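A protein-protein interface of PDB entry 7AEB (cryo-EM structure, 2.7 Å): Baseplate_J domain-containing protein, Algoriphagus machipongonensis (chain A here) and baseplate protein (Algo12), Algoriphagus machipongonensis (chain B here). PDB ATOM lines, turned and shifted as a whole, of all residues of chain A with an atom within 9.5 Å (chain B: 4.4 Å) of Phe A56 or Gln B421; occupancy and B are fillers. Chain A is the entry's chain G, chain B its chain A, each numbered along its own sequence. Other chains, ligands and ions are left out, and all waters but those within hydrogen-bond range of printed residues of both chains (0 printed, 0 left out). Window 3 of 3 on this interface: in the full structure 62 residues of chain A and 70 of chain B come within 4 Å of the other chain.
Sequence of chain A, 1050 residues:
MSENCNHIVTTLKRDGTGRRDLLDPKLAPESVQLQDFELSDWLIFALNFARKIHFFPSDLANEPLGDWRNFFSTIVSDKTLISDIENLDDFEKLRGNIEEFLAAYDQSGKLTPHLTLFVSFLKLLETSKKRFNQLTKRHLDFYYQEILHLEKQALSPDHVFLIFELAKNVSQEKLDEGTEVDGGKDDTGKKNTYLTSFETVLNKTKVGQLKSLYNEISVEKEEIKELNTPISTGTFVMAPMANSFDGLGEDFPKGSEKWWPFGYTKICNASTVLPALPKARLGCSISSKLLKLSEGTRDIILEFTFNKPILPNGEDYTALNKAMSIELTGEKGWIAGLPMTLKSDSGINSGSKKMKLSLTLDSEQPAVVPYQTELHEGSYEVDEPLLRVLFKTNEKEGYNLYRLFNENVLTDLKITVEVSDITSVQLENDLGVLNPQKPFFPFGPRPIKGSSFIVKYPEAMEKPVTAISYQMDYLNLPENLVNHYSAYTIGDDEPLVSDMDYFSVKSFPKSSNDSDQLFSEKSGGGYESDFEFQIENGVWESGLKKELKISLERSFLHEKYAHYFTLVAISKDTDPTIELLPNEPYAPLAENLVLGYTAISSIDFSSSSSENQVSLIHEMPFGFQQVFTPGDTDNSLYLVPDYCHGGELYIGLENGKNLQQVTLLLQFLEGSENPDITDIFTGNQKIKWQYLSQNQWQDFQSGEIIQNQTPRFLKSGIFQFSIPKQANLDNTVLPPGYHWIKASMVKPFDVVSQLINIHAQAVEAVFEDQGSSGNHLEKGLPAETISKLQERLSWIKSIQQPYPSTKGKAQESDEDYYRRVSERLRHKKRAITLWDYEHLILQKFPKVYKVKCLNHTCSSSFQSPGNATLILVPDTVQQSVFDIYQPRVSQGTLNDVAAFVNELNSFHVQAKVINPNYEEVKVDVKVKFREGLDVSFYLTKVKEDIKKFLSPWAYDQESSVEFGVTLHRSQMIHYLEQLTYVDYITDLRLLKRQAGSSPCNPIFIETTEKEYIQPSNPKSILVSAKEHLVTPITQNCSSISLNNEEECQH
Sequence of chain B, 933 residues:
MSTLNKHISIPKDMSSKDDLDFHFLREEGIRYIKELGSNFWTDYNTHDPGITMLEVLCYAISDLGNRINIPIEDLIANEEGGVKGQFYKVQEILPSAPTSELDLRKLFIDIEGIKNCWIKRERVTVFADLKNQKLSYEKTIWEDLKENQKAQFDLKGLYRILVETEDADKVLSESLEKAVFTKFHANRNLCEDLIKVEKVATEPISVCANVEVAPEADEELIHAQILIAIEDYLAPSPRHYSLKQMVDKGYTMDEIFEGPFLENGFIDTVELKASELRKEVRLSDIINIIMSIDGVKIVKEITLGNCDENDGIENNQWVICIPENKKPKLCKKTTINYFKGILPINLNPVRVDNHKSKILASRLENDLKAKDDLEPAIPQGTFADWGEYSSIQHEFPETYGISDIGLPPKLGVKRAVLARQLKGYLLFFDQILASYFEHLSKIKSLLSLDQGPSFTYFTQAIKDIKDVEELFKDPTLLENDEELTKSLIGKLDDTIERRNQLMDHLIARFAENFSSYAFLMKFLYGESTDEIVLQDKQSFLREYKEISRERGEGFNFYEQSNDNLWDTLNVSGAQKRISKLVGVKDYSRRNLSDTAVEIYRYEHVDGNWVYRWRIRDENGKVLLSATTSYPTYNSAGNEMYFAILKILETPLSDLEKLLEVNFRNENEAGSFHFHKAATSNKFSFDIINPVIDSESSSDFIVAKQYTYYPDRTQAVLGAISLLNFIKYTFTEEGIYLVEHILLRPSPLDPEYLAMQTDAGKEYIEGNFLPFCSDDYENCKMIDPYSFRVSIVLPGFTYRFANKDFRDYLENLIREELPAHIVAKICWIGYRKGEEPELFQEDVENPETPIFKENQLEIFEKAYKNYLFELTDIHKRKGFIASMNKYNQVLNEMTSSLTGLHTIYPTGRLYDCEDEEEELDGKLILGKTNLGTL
The side-chain amide nitrogen of Gln B421 lies within hydrogen-bond range of the backbone carbonyl oxygen of Phe A56 (2.9 Å).
O of His A54 lies within hydrogen-bond range of NE1 of Trp A68.
Among the printed residues, pairs that only touch across the chains: Asn A62 with Val B417, Phe A56 with Arg B420, Trp A68 with Gln B421, Leu A60 with Val B417 and Pro A57 with Val B417.
Of the printed residues of chain B, Phe A56 touches Arg B420 and Gln B421. Of the printed residues of chain B, Pro A57 touches Val B417 (3.7 Å). Ser A58 touches none of the printed residues of chain B. Of the printed residues of chain B, Leu A60 touches Val B417. Printed residues of chain B within 4 Å of Trp A68: Gln B421 (3.7 Å). Of the printed residues of chain A, Val B417 touches Pro A57, Leu A60 and Asn A62. Of the printed residues of chain A, Arg B420 touches Phe A56 (3.6 Å). Printed residues of chain A within 4 Å of Gln B421: Phe A56 (2.9 Å) and Trp A68 (3.7 Å). No residue of chain A comes within 4 Å of Gly B424. The nearest residue of chain B that does not touch Phe A56 is Val B417 (4.1 Å). The nearest printed residue of chain A that does not touch Gln B421 is Ser A58 (4.005 Å).
Printed residues of chain B that touch a printed residue of chain A: Val B417, Arg B420 and Gln B421. Hydrophobic or aromatic side chains of chain B within 4 Å of the printed part of chain A: Val B417. Hydrophobic or aromatic side chains of chain A within 4 Å of the printed part of chain B: Phe A56 and Trp A68. Among the printed residues, 6 pairs touch across the chains. Among the printed residues, no Asp or Glu carboxylate lies within 4 Å of a Lys or Arg side-chain nitrogen of the other chain.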
ATOM      1  N   ILE A  53       3.754  28.741  19.380  1.00  0.00           N
ATOM      2  CA  ILE A  53       4.755  28.646  18.325  1.00  0.00           C
ATOM      3  C   ILE A  53       4.146  27.911  17.132  1.00  0.00           C
ATOM      4  O   ILE A  53       3.543  26.852  17.305  1.00  0.00           O
ATOM      5  CB  ILE A  53       6.001  27.900  18.838  1.00  0.00           C
ATOM      6  CG1 ILE A  53       6.589  28.588  20.070  1.00  0.00           C
ATOM      7  CG2 ILE A  53       7.041  27.748  17.765  1.00  0.00           C
ATOM      8  CD1 ILE A  53       7.064  30.000  19.859  1.00  0.00           C
ATOM      9  N   HIS A  54       4.300  28.460  15.930  1.00  0.00           N
ATOM     10  CA  HIS A  54       3.818  27.847  14.691  1.00  0.00           C
ATOM     11  C   HIS A  54       4.618  26.592  14.377  1.00  0.00           C
ATOM     12  O   HIS A  54       5.723  26.433  14.868  1.00  0.00           O
ATOM     13  CB  HIS A  54       4.062  28.780  13.517  1.00  0.00           C
ATOM     14  CG  HIS A  54       3.042  29.857  13.328  1.00  0.00           C
ATOM     15  ND1 HIS A  54       3.387  31.139  12.961  1.00  0.00           N
ATOM     16  CD2 HIS A  54       1.692  29.838  13.393  1.00  0.00           C
ATOM     17  CE1 HIS A  54       2.299  31.869  12.834  1.00  0.00           C
ATOM     18  NE2 HIS A  54       1.257  31.102  13.093  1.00  0.00           N
ATOM     19  N   PHE A  55       4.063  25.678  13.575  1.00  0.00           N
ATOM     20  CA  PHE A  55       4.801  24.500  13.123  1.00  0.00           C
ATOM     21  C   PHE A  55       4.731  24.497  11.618  1.00  0.00           C
ATOM     22  O   PHE A  55       3.674  24.703  11.063  1.00  0.00           O
ATOM     23  CB  PHE A  55       4.254  23.185  13.631  1.00  0.00           C
ATOM     24  CG  PHE A  55       5.027  22.001  13.147  1.00  0.00           C
ATOM     25  CD1 PHE A  55       6.108  21.537  13.852  1.00  0.00           C
ATOM     26  CD2 PHE A  55       4.687  21.359  11.978  1.00  0.00           C
ATOM     27  CE1 PHE A  55       6.829  20.459  13.394  1.00  0.00           C
ATOM     28  CE2 PHE A  55       5.404  20.288  11.523  1.00  0.00           C
ATOM     29  CZ  PHE A  55       6.478  19.837  12.230  1.00  0.00           C
ATOM     30  N   PHE A  56       5.842  24.222  10.962  1.00  0.00           N
ATOM     31  CA  PHE A  56       5.911  24.260   9.500  1.00  0.00           C
ATOM     32  C   PHE A  56       6.123  22.887   8.876  1.00  0.00           C
ATOM     33  O   PHE A  56       7.240  22.361   8.941  1.00  0.00           O
ATOM     34  CB  PHE A  56       7.039  25.178   9.062  1.00  0.00           C
ATOM     35  CG  PHE A  56       6.805  26.586   9.376  1.00  0.00           C
ATOM     36  CD1 PHE A  56       7.158  27.111  10.595  1.00  0.00           C
ATOM     37  CD2 PHE A  56       6.231  27.396   8.444  1.00  0.00           C
ATOM     38  CE1 PHE A  56       6.925  28.423  10.872  1.00  0.00           C
ATOM     39  CE2 PHE A  56       6.004  28.706   8.710  1.00  0.00           C
ATOM     40  CZ  PHE A  56       6.345  29.223   9.922  1.00  0.00           C
ATOM     41  N   PRO A  57       5.101  22.311   8.239  1.00  0.00           N
ATOM     42  CA  PRO A  57       5.197  21.005   7.568  1.00  0.00           C
ATOM     43  C   PRO A  57       6.202  21.004   6.435  1.00  0.00           C
ATOM     44  O   PRO A  57       6.341  21.992   5.718  1.00  0.00           O
ATOM     45  CB  PRO A  57       3.785  20.807   7.016  1.00  0.00           C
ATOM     46  CG  PRO A  57       2.943  21.662   7.854  1.00  0.00           C
ATOM     47  CD  PRO A  57       3.746  22.848   8.209  1.00  0.00           C
ATOM     48  N   SER A  58       6.831  19.846   6.213  1.00  0.00           N
ATOM     49  CA  SER A  58       7.907  19.764   5.234  1.00  0.00           C
ATOM     50  C   SER A  58       7.380  19.808   3.792  1.00  0.00           C
ATOM     51  O   SER A  58       8.177  19.921   2.860  1.00  0.00           O
ATOM     52  CB  SER A  58       8.666  18.451   5.303  1.00  0.00           C
ATOM     53  OG  SER A  58       7.796  17.354   5.337  1.00  0.00           O
ATOM     54  N   ASP A  59       6.074  19.680   3.572  1.00  0.00           N
ATOM     55  CA  ASP A  59       5.531  19.707   2.222  1.00  0.00           C
ATOM     56  C   ASP A  59       4.919  21.053   1.832  1.00  0.00           C
ATOM     57  O   ASP A  59       4.311  21.155   0.764  1.00  0.00           O
ATOM     58  CB  ASP A  59       4.507  18.594   2.068  1.00  0.00           C
ATOM     59  CG  ASP A  59       3.448  18.661   3.119  1.00  0.00           C
ATOM     60  OD1 ASP A  59       3.607  19.462   4.046  1.00  0.00           O
ATOM     61  OD2 ASP A  59       2.460  17.933   3.030  1.00  0.00           O
ATOM     62  N   LEU A  60       5.068  22.085   2.649  1.00  0.00           N
ATOM     63  CA  LEU A  60       4.543  23.393   2.295  1.00  0.00           C
ATOM     64  C   LEU A  60       5.690  24.373   2.125  1.00  0.00           C
ATOM     65  O   LEU A  60       6.724  24.259   2.779  1.00  0.00           O
ATOM     66  CB  LEU A  60       3.567  23.901   3.354  1.00  0.00           C
ATOM     67  CG  LEU A  60       2.358  23.015   3.679  1.00  0.00           C
ATOM     68  CD1 LEU A  60       1.562  23.630   4.815  1.00  0.00           C
ATOM     69  CD2 LEU A  60       1.478  22.842   2.466  1.00  0.00           C
ATOM     70  N   ALA A  61       5.501  25.376   1.276  1.00  0.00           N
ATOM     71  CA  ALA A  61       6.553  26.363   1.040  1.00  0.00           C
ATOM     72  C   ALA A  61       6.608  27.387   2.165  1.00  0.00           C
ATOM     73  O   ALA A  61       6.274  28.558   1.978  1.00  0.00           O
ATOM     74  CB  ALA A  61       6.327  27.075  -0.278  1.00  0.00           C
ATOM     75  N   ASN A  62       7.067  26.923   3.317  1.00  0.00           N
ATOM     76  CA  ASN A  62       7.151  27.767   4.481  1.00  0.00           C
ATOM     77  C   ASN A  62       5.795  28.334   4.881  1.00  0.00           C
ATOM     78  O   ASN A  62       5.694  29.504   5.201  1.00  0.00           O
ATOM     79  CB  ASN A  62       8.158  28.891   4.251  1.00  0.00           C
ATOM     80  CG  ASN A  62       9.556  28.488   4.604  1.00  0.00           C
ATOM     81  OD1 ASN A  62       9.759  27.552   5.366  1.00  0.00           O
ATOM     82  ND2 ASN A  62      10.533  29.198   4.066  1.00  0.00           N
ATOM     83  N   GLU A  63       4.746  27.528   4.827  1.00  0.00           N
ATOM     84  CA  GLU A  63       3.461  27.999   5.284  1.00  0.00           C
ATOM     85  C   GLU A  63       3.221  27.309   6.616  1.00  0.00           C
ATOM     86  O   GLU A  63       3.585  26.145   6.760  1.00  0.00           O
ATOM     87  CB  GLU A  63       2.375  27.572   4.302  1.00  0.00           C
ATOM     88  CG  GLU A  63       2.423  28.251   2.968  1.00  0.00           C
ATOM     89  CD  GLU A  63       1.410  27.677   2.020  1.00  0.00           C
ATOM     90  OE1 GLU A  63       0.641  26.808   2.443  1.00  0.00           O
ATOM     91  OE2 GLU A  63       1.331  28.132   0.875  1.00  0.00           O
ATOM     92  N   PRO A  64       2.677  27.993   7.609  1.00  0.00           N
ATOM     93  CA  PRO A  64       2.407  27.381   8.914  1.00  0.00           C
ATOM     94  C   PRO A  64       1.170  26.504   8.862  1.00  0.00           C
ATOM     95  O   PRO A  64       0.252  26.757   8.086  1.00  0.00           O
ATOM     96  CB  PRO A  64       2.169  28.602   9.805  1.00  0.00           C
ATOM     97  CG  PRO A  64       1.630  29.634   8.851  1.00  0.00           C
ATOM     98  CD  PRO A  64       2.312  29.406   7.550  1.00  0.00           C
ATOM     99  N   LEU A  65       1.148  25.460   9.703  1.00  0.00           N
ATOM    100  CA  LEU A  65      -0.051  24.625   9.835  1.00  0.00           C
ATOM    101  C   LEU A  65      -0.096  23.974  11.222  1.00  0.00           C
ATOM    102  O   LEU A  65       0.298  22.821  11.392  1.00  0.00           O
ATOM    103  CB  LEU A  65      -0.057  23.554   8.754  1.00  0.00           C
ATOM    104  CG  LEU A  65      -1.287  22.657   8.630  1.00  0.00           C
ATOM    105  CD1 LEU A  65      -2.495  23.478   8.261  1.00  0.00           C
ATOM    106  CD2 LEU A  65      -1.021  21.589   7.603  1.00  0.00           C
ATOM    107  N   GLY A  66      -0.655  24.668  12.197  1.00  0.00           N
ATOM    108  CA  GLY A  66      -0.703  24.108  13.542  1.00  0.00           C
ATOM    109  C   GLY A  66       0.478  24.525  14.399  1.00  0.00           C
ATOM    110  O   GLY A  66       1.154  25.517  14.118  1.00  0.00           O
ATOM    111  N   ASP A  67       0.735  23.746  15.446  1.00  0.00           N
ATOM    112  CA  ASP A  67       1.707  24.105  16.482  1.00  0.00           C
ATOM    113  C   ASP A  67       2.532  22.876  16.878  1.00  0.00           C
ATOM    114  O   ASP A  67       2.534  21.851  16.190  1.00  0.00           O
ATOM    115  CB  ASP A  67       0.977  24.748  17.668  1.00  0.00           C
ATOM    116  CG  ASP A  67      -0.025  23.819  18.309  1.00  0.00           C
ATOM    117  OD1 ASP A  67       0.043  22.616  18.111  1.00  0.00           O
ATOM    118  OD2 ASP A  67      -0.936  24.278  19.001  1.00  0.00           O
ATOM    119  N   TRP A  68       3.160  22.939  18.049  1.00  0.00           N
ATOM    120  CA  TRP A  68       4.040  21.896  18.554  1.00  0.00           C
ATOM    121  C   TRP A  68       3.400  21.066  19.651  1.00  0.00           C
ATOM    122  O   TRP A  68       4.098  20.354  20.377  1.00  0.00           O
ATOM    123  CB  TRP A  68       5.314  22.548  19.058  1.00  0.00           C
ATOM    124  CG  TRP A  68       6.125  23.087  17.971  1.00  0.00           C
ATOM    125  CD1 TRP A  68       5.929  24.241  17.288  1.00  0.00           C
ATOM    126  CD2 TRP A  68       7.289  22.499  17.436  1.00  0.00           C
ATOM    127  NE1 TRP A  68       6.899  24.401  16.351  1.00  0.00           N
ATOM    128  CE2 TRP A  68       7.751  23.339  16.428  1.00  0.00           C
ATOM    129  CE3 TRP A  68       7.993  21.336  17.719  1.00  0.00           C
ATOM    130  CZ2 TRP A  68       8.870  23.052  15.705  1.00  0.00           C
ATOM    131  CZ3 TRP A  68       9.103  21.059  17.004  1.00  0.00           C
ATOM    132  CH2 TRP A  68       9.535  21.903  16.011  1.00  0.00           C
ATOM    133  N   PHE A  71       4.160  17.256  20.513  1.00  0.00           N
ATOM    134  CA  PHE A  71       5.477  16.796  20.888  1.00  0.00           C
ATOM    135  C   PHE A  71       5.637  16.631  22.392  1.00  0.00           C
ATOM    136  O   PHE A  71       6.625  16.039  22.832  1.00  0.00           O
ATOM    137  CB  PHE A  71       6.512  17.755  20.309  1.00  0.00           C
ATOM    138  CG  PHE A  71       6.615  17.681  18.805  1.00  0.00           C
ATOM    139  CD1 PHE A  71       5.821  18.471  18.003  1.00  0.00           C
ATOM    140  CD2 PHE A  71       7.499  16.812  18.199  1.00  0.00           C
ATOM    141  CE1 PHE A  71       5.909  18.401  16.636  1.00  0.00           C
ATOM    142  CE2 PHE A  71       7.589  16.749  16.833  1.00  0.00           C
ATOM    143  CZ  PHE A  71       6.791  17.539  16.054  1.00  0.00           C
ATOM    144  N   VAL B 417      13.122  24.727   4.667  1.00  0.00           N
ATOM    145  CA  VAL B 417      12.011  24.474   5.579  1.00  0.00           C
ATOM    146  C   VAL B 417      12.485  23.767   6.821  1.00  0.00           C
ATOM    147  O   VAL B 417      12.065  24.098   7.936  1.00  0.00           O
ATOM    148  CB  VAL B 417      10.919  23.636   4.909  1.00  0.00           C
ATOM    149  CG1 VAL B 417       9.879  23.202   5.939  1.00  0.00           C
ATOM    150  CG2 VAL B 417      10.271  24.450   3.835  1.00  0.00           C
ATOM    151  N   LEU B 418      13.328  22.760   6.641  1.00  0.00           N
ATOM    152  CA  LEU B 418      13.836  22.015   7.770  1.00  0.00           C
ATOM    153  C   LEU B 418      14.638  22.913   8.698  1.00  0.00           C
ATOM    154  O   LEU B 418      14.636  22.705   9.913  1.00  0.00           O
ATOM    155  CB  LEU B 418      14.685  20.854   7.281  1.00  0.00           C
ATOM    156  CG  LEU B 418      13.944  19.732   6.525  1.00  0.00           C
ATOM    157  CD1 LEU B 418      14.952  18.767   5.972  1.00  0.00           C
ATOM    158  CD2 LEU B 418      12.968  19.011   7.423  1.00  0.00           C
ATOM    159  N   ALA B 419      15.348  23.896   8.145  1.00  0.00           N
ATOM    160  CA  ALA B 419      16.073  24.822   9.000  1.00  0.00           C
ATOM    161  C   ALA B 419      15.113  25.583   9.899  1.00  0.00           C
ATOM    162  O   ALA B 419      15.394  25.775  11.088  1.00  0.00           O
ATOM    163  CB  ALA B 419      16.885  25.786   8.168  1.00  0.00           C
ATOM    164  N   ARG B 420      13.950  25.960   9.352  1.00  0.00           N
ATOM    165  CA  ARG B 420      12.918  26.668  10.119  1.00  0.00           C
ATOM    166  C   ARG B 420      12.440  25.801  11.274  1.00  0.00           C
ATOM    167  O   ARG B 420      12.262  26.313  12.391  1.00  0.00           O
ATOM    168  CB  ARG B 420      11.744  27.049   9.208  1.00  0.00           C
ATOM    169  CG  ARG B 420      10.633  27.827   9.894  1.00  0.00           C
ATOM    170  CD  ARG B 420      11.095  29.189  10.358  1.00  0.00           C
ATOM    171  NE  ARG B 420      11.547  30.030   9.264  1.00  0.00           N
ATOM    172  CZ  ARG B 420      10.756  30.824   8.553  1.00  0.00           C
ATOM    173  NH1 ARG B 420      11.260  31.553   7.572  1.00  0.00           N
ATOM    174  NH2 ARG B 420       9.466  30.891   8.827  1.00  0.00           N
ATOM    175  N   GLN B 421      12.283  24.488  11.026  1.00  0.00           N
ATOM    176  CA  GLN B 421      11.818  23.568  12.057  1.00  0.00           C
ATOM    177  C   GLN B 421      12.809  23.489  13.200  1.00  0.00           C
ATOM    178  O   GLN B 421      12.416  23.481  14.374  1.00  0.00           O
ATOM    179  CB  GLN B 421      11.605  22.166  11.500  1.00  0.00           C
ATOM    180  CG  GLN B 421      10.471  22.020  10.553  1.00  0.00           C
ATOM    181  CD  GLN B 421      10.360  20.621  10.063  1.00  0.00           C
ATOM    182  OE1 GLN B 421      11.211  19.796  10.363  1.00  0.00           O
ATOM    183  NE2 GLN B 421       9.322  20.332   9.311  1.00  0.00           N
ATOM    184  N   LEU B 422      14.105  23.471  12.875  1.00  0.00           N
ATOM    185  CA  LEU B 422      15.120  23.428  13.914  1.00  0.00           C
ATOM    186  C   LEU B 422      15.116  24.696  14.749  1.00  0.00           C
ATOM    187  O   LEU B 422      15.243  24.611  15.972  1.00  0.00           O
ATOM    188  CB  LEU B 422      16.514  23.181  13.335  1.00  0.00           C
ATOM    189  CG  LEU B 422      17.686  23.106  14.363  1.00  0.00           C
ATOM    190  CD1 LEU B 422      17.456  21.999  15.383  1.00  0.00           C
ATOM    191  CD2 LEU B 422      18.999  22.875  13.635  1.00  0.00           C
ATOM    192  N   LYS B 423      14.964  25.870  14.127  1.00  0.00           N
ATOM    193  CA  LYS B 423      14.940  27.103  14.914  1.00  0.00           C
ATOM    194  C   LYS B 423      13.844  27.049  15.959  1.00  0.00           C
ATOM    195  O   LYS B 423      14.064  27.414  17.118  1.00  0.00           O
ATOM    196  CB  LYS B 423      14.699  28.323  14.041  1.00  0.00           C
ATOM    197  CG  LYS B 423      15.824  28.665  13.152  1.00  0.00           C
ATOM    198  CD  LYS B 423      15.523  29.873  12.318  1.00  0.00           C
ATOM    199  CE  LYS B 423      16.643  30.131  11.362  1.00  0.00           C
ATOM    200  NZ  LYS B 423      16.403  31.323  10.541  1.00  0.00           N
ATOM    201  N   GLY B 424      12.680  26.534  15.558  1.00  0.00           N
ATOM    202  CA  GLY B 424      11.563  26.391  16.467  1.00  0.00           C
ATOM    203  C   GLY B 424      11.939  25.555  17.668  1.00  0.00           C
ATOM    204  O   GLY B 424      11.748  25.966  18.807  1.00  0.00           O
ATOM    205  N   TYR B 425      12.502  24.385  17.416  1.00  0.00           N
ATOM    206  CA  TYR B 425      12.913  23.485  18.483  1.00  0.00           C
ATOM    207  C   TYR B 425      13.896  24.141  19.432  1.00  0.00           C
ATOM    208  O   TYR B 425      13.721  24.100  20.648  1.00  0.00           O
ATOM    209  CB  TYR B 425      13.512  22.228  17.875  1.00  0.00           C
ATOM    210  CG  TYR B 425      14.049  21.232  18.849  1.00  0.00           C
ATOM    211  CD1 TYR B 425      13.196  20.439  19.568  1.00  0.00           C
ATOM    212  CD2 TYR B 425      15.406  21.066  19.002  1.00  0.00           C
ATOM    213  CE1 TYR B 425      13.678  19.512  20.431  1.00  0.00           C
ATOM    214  CE2 TYR B 425      15.893  20.135  19.862  1.00  0.00           C
ATOM    215  CZ  TYR B 425      15.027  19.359  20.576  1.00  0.00           C
ATOM    216  OH  TYR B 425      15.509  18.424  21.445  1.00  0.00           O
